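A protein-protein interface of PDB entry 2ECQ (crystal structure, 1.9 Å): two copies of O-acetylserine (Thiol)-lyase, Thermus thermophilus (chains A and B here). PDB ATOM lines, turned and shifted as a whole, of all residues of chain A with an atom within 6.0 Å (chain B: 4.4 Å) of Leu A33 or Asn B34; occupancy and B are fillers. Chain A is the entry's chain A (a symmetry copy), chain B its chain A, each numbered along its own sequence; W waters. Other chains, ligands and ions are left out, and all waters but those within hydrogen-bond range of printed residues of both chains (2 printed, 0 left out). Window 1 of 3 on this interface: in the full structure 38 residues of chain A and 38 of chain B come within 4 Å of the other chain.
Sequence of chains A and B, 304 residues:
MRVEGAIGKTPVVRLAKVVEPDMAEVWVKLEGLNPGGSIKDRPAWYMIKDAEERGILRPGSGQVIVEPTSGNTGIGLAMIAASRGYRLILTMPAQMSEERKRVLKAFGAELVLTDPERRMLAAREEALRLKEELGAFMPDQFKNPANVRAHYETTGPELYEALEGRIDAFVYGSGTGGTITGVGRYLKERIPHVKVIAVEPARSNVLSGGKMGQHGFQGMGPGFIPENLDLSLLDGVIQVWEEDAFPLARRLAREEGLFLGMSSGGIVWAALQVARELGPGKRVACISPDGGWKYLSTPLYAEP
The backbone NH of Gly B8 lies within hydrogen-bond range of the side-chain amide oxygen of Asn B34, 2.8 Å away. The side-chain amide nitrogen (ND2) of Asn B34 is in hydrogen-bond range of the backbone carbonyl oxygen (O) of Glu B31. O of Ser B38 lies within hydrogen-bond range of ND2 of Asn B34 (3.3 Å). N of Gly B36 sits at hydrogen-bond distance from OD2 of Asp B41, at 2.6 Å. The side-chain amide oxygen of Asn A34 lies within hydrogen-bond range of the backbone NH of Gly A8 (2.8 Å). ND2 of Asn A34 sits at hydrogen-bond distance from O of Glu A31.
Among the printed residues, merely in contact across the chains: Leu A33 with Leu B33, Leu A33 with Asn B34, Leu A33 with Pro B35, Asn A34 with Leu B33, Pro A35 with Leu B33, Trp A293 with Gly B36 and Trp A293 with Gly B37.
Printed residues of chain B within 4 Å of Asn A34: Leu B33 (3.7 Å). Printed residues of chain B within 4 Å of Pro A35: Leu B33 (3.7 Å). Of chain A, only Leu A33 (3.7 Å) comes within 4 Å of Asn B34. Printed residues of chain A within 4 Å of Pro B35: Leu A33. Printed residues of chain A within 4 Å of Gly B36: Trp A293. The nearest printed residue of chain B that does not touch Leu A33 is Gly B36 (5.7 Å). The nearest residue of chain A that does not touch Asn B34 is Trp A293 (5.7 Å). The nearest printed residue of chain A that does not touch Pro B35 is Trp A293 (4.2 Å).
Printed residues of chain A that touch a printed residue of chain B: Leu A33, Asn A34, Pro A35 and Trp A293. Hydrophobic or aromatic side chains of chain A within 4 Å of the printed part of chain B: Leu A33 and Trp A293. Along chain A the printed residues that touch a printed residue of chain B span positions 33 to 293. Hydrophobic or aromatic side chains of chain B that line the printed part of chain A: Leu B33. Along chain B the printed residues that touch a printed residue of chain A span positions 33 to 37. Among the printed residues, 7 pairs touch across the chains.
Leu B33 touches its own counterpart, Leu A33. Leu A33 touches Asn B34, and with the chains exchanged Asn A34 touches Leu B33. Leu A33 touches Pro B35, and with the chains exchanged Pro A35 touches Leu B33. Of the 7 pairs that touch across the chains among the printed residues, 5 have their exchanged pair printed and touching as well.
Water W1 bridges O of Pro B35 (2.7 Å) and NE1 of Trp A293 (3.1 Å). Water W2 lies within hydrogen-bond range of O of Asn B34 (3.0 Å) and NE1 of Trp A293 (3.4 Å).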
ATOM      1  N   ALA A   6      -0.038  30.055  14.235  1.00  0.00           N
ATOM      2  CA  ALA A   6       0.058  28.608  14.422  1.00  0.00           C
ATOM      3  C   ALA A   6       1.067  27.968  13.466  1.00  0.00           C
ATOM      4  O   ALA A   6       1.204  26.740  13.420  1.00  0.00           O
ATOM      5  CB  ALA A   6      -1.312  27.973  14.228  1.00  0.00           C
ATOM      6  N   GLY A   8       4.722  26.912  12.049  1.00  0.00           N
ATOM      7  CA  GLY A   8       6.020  26.566  12.603  1.00  0.00           C
ATOM      8  C   GLY A   8       6.042  25.676  13.830  1.00  0.00           C
ATOM      9  O   GLY A   8       5.034  25.069  14.197  1.00  0.00           O
ATOM     10  N   THR A  10       7.351  22.843  14.235  1.00  0.00           N
ATOM     11  CA  THR A  10       7.004  21.487  13.831  1.00  0.00           C
ATOM     12  C   THR A  10       7.952  20.465  14.449  1.00  0.00           C
ATOM     13  O   THR A  10       9.120  20.759  14.704  1.00  0.00           O
ATOM     14  CB  THR A  10       7.064  21.347  12.306  1.00  0.00           C
ATOM     15  OG1 THR A  10       8.368  21.730  11.852  1.00  0.00           O
ATOM     16  CG2 THR A  10       6.012  22.236  11.644  1.00  0.00           C
ATOM     17  N   PRO A  11       7.462  19.237  14.676  1.00  0.00           N
ATOM     18  CA  PRO A  11       8.275  18.173  15.270  1.00  0.00           C
ATOM     19  C   PRO A  11       9.222  17.475  14.301  1.00  0.00           C
ATOM     20  O   PRO A  11       9.062  17.544  13.079  1.00  0.00           O
ATOM     21  CB  PRO A  11       7.225  17.219  15.818  1.00  0.00           C
ATOM     22  CG  PRO A  11       6.170  17.288  14.758  1.00  0.00           C
ATOM     23  CD  PRO A  11       6.072  18.781  14.476  1.00  0.00           C
ATOM     24  N   LEU A  30       8.644  17.336  10.166  1.00  0.00           N
ATOM     25  CA  LEU A  30       7.327  17.258   9.533  1.00  0.00           C
ATOM     26  C   LEU A  30       6.615  18.590   9.306  1.00  0.00           C
ATOM     27  O   LEU A  30       5.837  19.039  10.150  1.00  0.00           O
ATOM     28  CB  LEU A  30       6.434  16.325  10.364  1.00  0.00           C
ATOM     29  CG  LEU A  30       7.091  14.977  10.697  1.00  0.00           C
ATOM     30  CD1 LEU A  30       6.194  14.170  11.623  1.00  0.00           C
ATOM     31  CD2 LEU A  30       7.365  14.207   9.407  1.00  0.00           C
ATOM     32  N   GLU A  31       6.861  19.200   8.150  1.00  0.00           N
ATOM     33  CA  GLU A  31       6.253  20.490   7.819  1.00  0.00           C
ATOM     34  C   GLU A  31       4.802  20.394   7.361  1.00  0.00           C
ATOM     35  O   GLU A  31       4.130  21.411   7.169  1.00  0.00           O
ATOM     36  CB  GLU A  31       7.099  21.199   6.760  1.00  0.00           C
ATOM     37  CG  GLU A  31       8.454  21.642   7.309  1.00  0.00           C
ATOM     38  CD  GLU A  31       8.314  22.717   8.371  1.00  0.00           C
ATOM     39  OE1 GLU A  31       8.944  22.595   9.442  1.00  0.00           O
ATOM     40  OE2 GLU A  31       7.571  23.691   8.130  1.00  0.00           O
ATOM     41  N   GLY A  32       4.320  19.170   7.190  1.00  0.00           N
ATOM     42  CA  GLY A  32       2.940  18.983   6.787  1.00  0.00           C
ATOM     43  C   GLY A  32       2.004  19.290   7.945  1.00  0.00           C
ATOM     44  O   GLY A  32       0.793  19.400   7.759  1.00  0.00           O
ATOM     45  N   LEU A  33       2.561  19.444   9.142  1.00  0.00           N
ATOM     46  CA  LEU A  33       1.741  19.731  10.315  1.00  0.00           C
ATOM     47  C   LEU A  33       1.483  21.223  10.511  1.00  0.00           C
ATOM     48  O   LEU A  33       1.162  21.671  11.606  1.00  0.00           O
ATOM     49  CB  LEU A  33       2.381  19.131  11.574  1.00  0.00           C
ATOM     50  CG  LEU A  33       2.575  17.609  11.528  1.00  0.00           C
ATOM     51  CD1 LEU A  33       3.133  17.119  12.852  1.00  0.00           C
ATOM     52  CD2 LEU A  33       1.244  16.926  11.236  1.00  0.00           C
ATOM     53  N   ASN A  34       1.626  21.993   9.440  1.00  0.00           N
ATOM     54  CA  ASN A  34       1.368  23.426   9.496  1.00  0.00           C
ATOM     55  C   ASN A  34      -0.099  23.625   9.138  1.00  0.00           C
ATOM     56  O   ASN A  34      -0.696  22.780   8.465  1.00  0.00           O
ATOM     57  CB  ASN A  34       2.274  24.170   8.510  1.00  0.00           C
ATOM     58  CG  ASN A  34       3.654  24.430   9.079  1.00  0.00           C
ATOM     59  OD1 ASN A  34       3.790  25.074  10.118  1.00  0.00           O
ATOM     60  ND2 ASN A  34       4.685  23.929   8.404  1.00  0.00           N
ATOM     61  N   PRO A  35      -0.705  24.739   9.583  1.00  0.00           N
ATOM     62  CA  PRO A  35      -2.118  25.007   9.291  1.00  0.00           C
ATOM     63  C   PRO A  35      -2.490  24.997   7.813  1.00  0.00           C
ATOM     64  O   PRO A  35      -3.621  24.667   7.457  1.00  0.00           O
ATOM     65  CB  PRO A  35      -2.364  26.365   9.956  1.00  0.00           C
ATOM     66  CG  PRO A  35      -1.008  27.007   9.957  1.00  0.00           C
ATOM     67  CD  PRO A  35      -0.098  25.860  10.323  1.00  0.00           C
ATOM     68  N   GLY A  37      -0.964  23.119   5.720  1.00  0.00           N
ATOM     69  CA  GLY A  37      -0.627  21.792   5.234  1.00  0.00           C
ATOM     70  C   GLY A  37       0.768  21.578   4.679  1.00  0.00           C
ATOM     71  O   GLY A  37       1.080  20.472   4.237  1.00  0.00           O
ATOM     72  N   SER A  38       1.620  22.600   4.696  1.00  0.00           N
ATOM     73  CA  SER A  38       2.966  22.426   4.157  1.00  0.00           C
ATOM     74  C   SER A  38       3.969  23.458   4.645  1.00  0.00           C
ATOM     75  O   SER A  38       3.616  24.444   5.298  1.00  0.00           O
ATOM     76  CB  SER A  38       2.941  22.487   2.631  1.00  0.00           C
ATOM     77  OG  SER A  38       2.961  23.840   2.191  1.00  0.00           O
ATOM     78  N   TRP A 293      -1.907  13.809   2.422  1.00  0.00           N
ATOM     79  CA  TRP A 293      -3.311  14.198   2.291  1.00  0.00           C
ATOM     80  C   TRP A 293      -3.789  14.738   0.944  1.00  0.00           C
ATOM     81  O   TRP A 293      -4.905  14.440   0.521  1.00  0.00           O
ATOM     82  CB  TRP A 293      -3.674  15.194   3.397  1.00  0.00           C
ATOM     83  CG  TRP A 293      -3.305  14.677   4.742  1.00  0.00           C
ATOM     84  CD1 TRP A 293      -2.195  14.998   5.468  1.00  0.00           C
ATOM     85  CD2 TRP A 293      -3.985  13.655   5.479  1.00  0.00           C
ATOM     86  NE1 TRP A 293      -2.138  14.233   6.610  1.00  0.00           N
ATOM     87  CE2 TRP A 293      -3.225  13.399   6.641  1.00  0.00           C
ATOM     88  CE3 TRP A 293      -5.163  12.924   5.266  1.00  0.00           C
ATOM     89  CZ2 TRP A 293      -3.603  12.444   7.589  1.00  0.00           C
ATOM     90  CZ3 TRP A 293      -5.541  11.973   6.212  1.00  0.00           C
ATOM     91  CH2 TRP A 293      -4.761  11.743   7.357  1.00  0.00           C
ATOM     92  N   ILE B   7       2.141  13.678  18.609  1.00  0.00           N
ATOM     93  CA  ILE B   7       0.717  13.873  18.872  1.00  0.00           C
ATOM     94  C   ILE B   7       0.479  14.895  19.983  1.00  0.00           C
ATOM     95  O   ILE B   7       1.171  14.885  21.000  1.00  0.00           O
ATOM     96  CB  ILE B   7       0.043  12.546  19.300  1.00  0.00           C
ATOM     97  CG1 ILE B   7       0.065  11.544  18.141  1.00  0.00           C
ATOM     98  CG2 ILE B   7      -1.391  12.808  19.758  1.00  0.00           C
ATOM     99  CD1 ILE B   7      -0.463  10.167  18.518  1.00  0.00           C
ATOM    100  N   GLY B   8      -0.496  15.778  19.781  1.00  0.00           N
ATOM    101  CA  GLY B   8      -0.826  16.761  20.798  1.00  0.00           C
ATOM    102  C   GLY B   8      -0.146  18.113  20.711  1.00  0.00           C
ATOM    103  O   GLY B   8       0.463  18.458  19.696  1.00  0.00           O
ATOM    104  N   THR B  10      -1.405  20.979  20.386  1.00  0.00           N
ATOM    105  CA  THR B  10      -1.990  21.721  19.277  1.00  0.00           C
ATOM    106  C   THR B  10      -2.310  23.158  19.679  1.00  0.00           C
ATOM    107  O   THR B  10      -2.605  23.438  20.841  1.00  0.00           O
ATOM    108  CB  THR B  10      -3.283  21.050  18.801  1.00  0.00           C
ATOM    109  OG1 THR B  10      -4.184  20.932  19.909  1.00  0.00           O
ATOM    110  CG2 THR B  10      -2.988  19.662  18.233  1.00  0.00           C
ATOM    111  N   GLU B  31      -7.191  20.489  16.285  1.00  0.00           N
ATOM    112  CA  GLU B  31      -6.729  19.103  16.379  1.00  0.00           C
ATOM    113  C   GLU B  31      -6.388  18.469  15.036  1.00  0.00           C
ATOM    114  O   GLU B  31      -5.870  17.350  14.977  1.00  0.00           O
ATOM    115  CB  GLU B  31      -7.774  18.263  17.115  1.00  0.00           C
ATOM    116  CG  GLU B  31      -7.882  18.642  18.590  1.00  0.00           C
ATOM    117  CD  GLU B  31      -6.615  18.308  19.357  1.00  0.00           C
ATOM    118  OE1 GLU B  31      -6.119  19.171  20.112  1.00  0.00           O
ATOM    119  OE2 GLU B  31      -6.114  17.175  19.205  1.00  0.00           O
ATOM    120  N   GLY B  32      -6.675  19.186  13.958  1.00  0.00           N
ATOM    121  CA  GLY B  32      -6.356  18.674  12.639  1.00  0.00           C
ATOM    122  C   GLY B  32      -4.857  18.738  12.396  1.00  0.00           C
ATOM    123  O   GLY B  32      -4.354  18.162  11.432  1.00  0.00           O
ATOM    124  N   LEU B  33      -4.134  19.427  13.274  1.00  0.00           N
ATOM    125  CA  LEU B  33      -2.688  19.552  13.117  1.00  0.00           C
ATOM    126  C   LEU B  33      -1.918  18.397  13.753  1.00  0.00           C
ATOM    127  O   LEU B  33      -0.737  18.516  14.055  1.00  0.00           O
ATOM    128  CB  LEU B  33      -2.204  20.892  13.684  1.00  0.00           C
ATOM    129  CG  LEU B  33      -2.831  22.128  13.025  1.00  0.00           C
ATOM    130  CD1 LEU B  33      -2.218  23.390  13.604  1.00  0.00           C
ATOM    131  CD2 LEU B  33      -2.610  22.082  11.519  1.00  0.00           C
ATOM    132  N   ASN B  34      -2.596  17.275  13.956  1.00  0.00           N
ATOM    133  CA  ASN B  34      -1.957  16.093  14.519  1.00  0.00           C
ATOM    134  C   ASN B  34      -1.432  15.274  13.347  1.00  0.00           C
ATOM    135  O   ASN B  34      -1.939  15.392  12.229  1.00  0.00           O
ATOM    136  CB  ASN B  34      -2.963  15.283  15.342  1.00  0.00           C
ATOM    137  CG  ASN B  34      -3.126  15.824  16.748  1.00  0.00           C
ATOM    138  OD1 ASN B  34      -2.158  15.907  17.502  1.00  0.00           O
ATOM    139  ND2 ASN B  34      -4.351  16.197  17.108  1.00  0.00           N
ATOM    140  N   PRO B  35      -0.408  14.434  13.581  1.00  0.00           N
ATOM    141  CA  PRO B  35       0.164  13.613  12.507  1.00  0.00           C
ATOM    142  C   PRO B  35      -0.830  12.723  11.769  1.00  0.00           C
ATOM    143  O   PRO B  35      -0.646  12.430  10.588  1.00  0.00           O
ATOM    144  CB  PRO B  35       1.260  12.814  13.221  1.00  0.00           C
ATOM    145  CG  PRO B  35       0.779  12.749  14.640  1.00  0.00           C
ATOM    146  CD  PRO B  35       0.237  14.138  14.872  1.00  0.00           C
ATOM    147  N   GLY B  36      -1.874  12.294  12.469  1.00  0.00           N
ATOM    148  CA  GLY B  36      -2.881  11.450  11.857  1.00  0.00           C
ATOM    149  C   GLY B  36      -3.993  12.278  11.242  1.00  0.00           C
ATOM    150  O   GLY B  36      -4.942  11.738  10.673  1.00  0.00           O
ATOM    151  N   GLY B  37      -3.883  13.596  11.382  1.00  0.00           N
ATOM    152  CA  GLY B  37      -4.873  14.493  10.811  1.00  0.00           C
ATOM    153  C   GLY B  37      -6.094  14.822  11.647  1.00  0.00           C
ATOM    154  O   GLY B  37      -6.963  15.561  11.184  1.00  0.00           O
ATOM    155  N   SER B  38      -6.182  14.302  12.869  1.00  0.00           N
ATOM    156  CA  SER B  38      -7.353  14.592  13.693  1.00  0.00           C
ATOM    157  C   SER B  38      -7.139  14.361  15.180  1.00  0.00           C
ATOM    158  O   SER B  38      -6.120  13.814  15.609  1.00  0.00           O
ATOM    159  CB  SER B  38      -8.538  13.734  13.254  1.00  0.00           C
ATOM    160  OG  SER B  38      -8.461  12.445  13.851  1.00  0.00           O
ATOM    161  N   ILE B  39      -8.135  14.772  15.953  1.00  0.00           N
ATOM    162  CA  ILE B  39      -8.122  14.621  17.401  1.00  0.00           C
ATOM    163  C   ILE B  39      -8.039  13.147  17.819  1.00  0.00           C
ATOM    164  O   ILE B  39      -7.575  12.838  18.918  1.00  0.00           O
ATOM    165  CB  ILE B  39      -9.397  15.257  18.013  1.00  0.00           C
ATOM    166  CG1 ILE B  39      -9.308  15.273  19.539  1.00  0.00           C
ATOM    167  CG2 ILE B  39     -10.632  14.486  17.559  1.00  0.00           C
ATOM    168  CD1 ILE B  39     -10.440  16.047  20.194  1.00  0.00           C
ATOM    169  N   ASP B  41      -6.033  10.952  17.087  1.00  0.00           N
ATOM    170  CA  ASP B  41      -4.672  10.467  17.303  1.00  0.00           C
ATOM    171  C   ASP B  41      -4.483  10.210  18.804  1.00  0.00           C
ATOM    172  O   ASP B  41      -3.831   9.245  19.208  1.00  0.00           O
ATOM    173  CB  ASP B  41      -3.645  11.520  16.875  1.00  0.00           C
ATOM    174  CG  ASP B  41      -3.393  11.533  15.382  1.00  0.00           C
ATOM    175  OD1 ASP B  41      -4.198  10.962  14.619  1.00  0.00           O
ATOM    176  OD2 ASP B  41      -2.377  12.137  14.977  1.00  0.00           O
HETATM  177  O   HOH W   1       0.249  13.919   8.538  1.00  0.00           O
HETATM  178  O   HOH W   2      -1.712  16.204   9.369  1.00  0.00           O
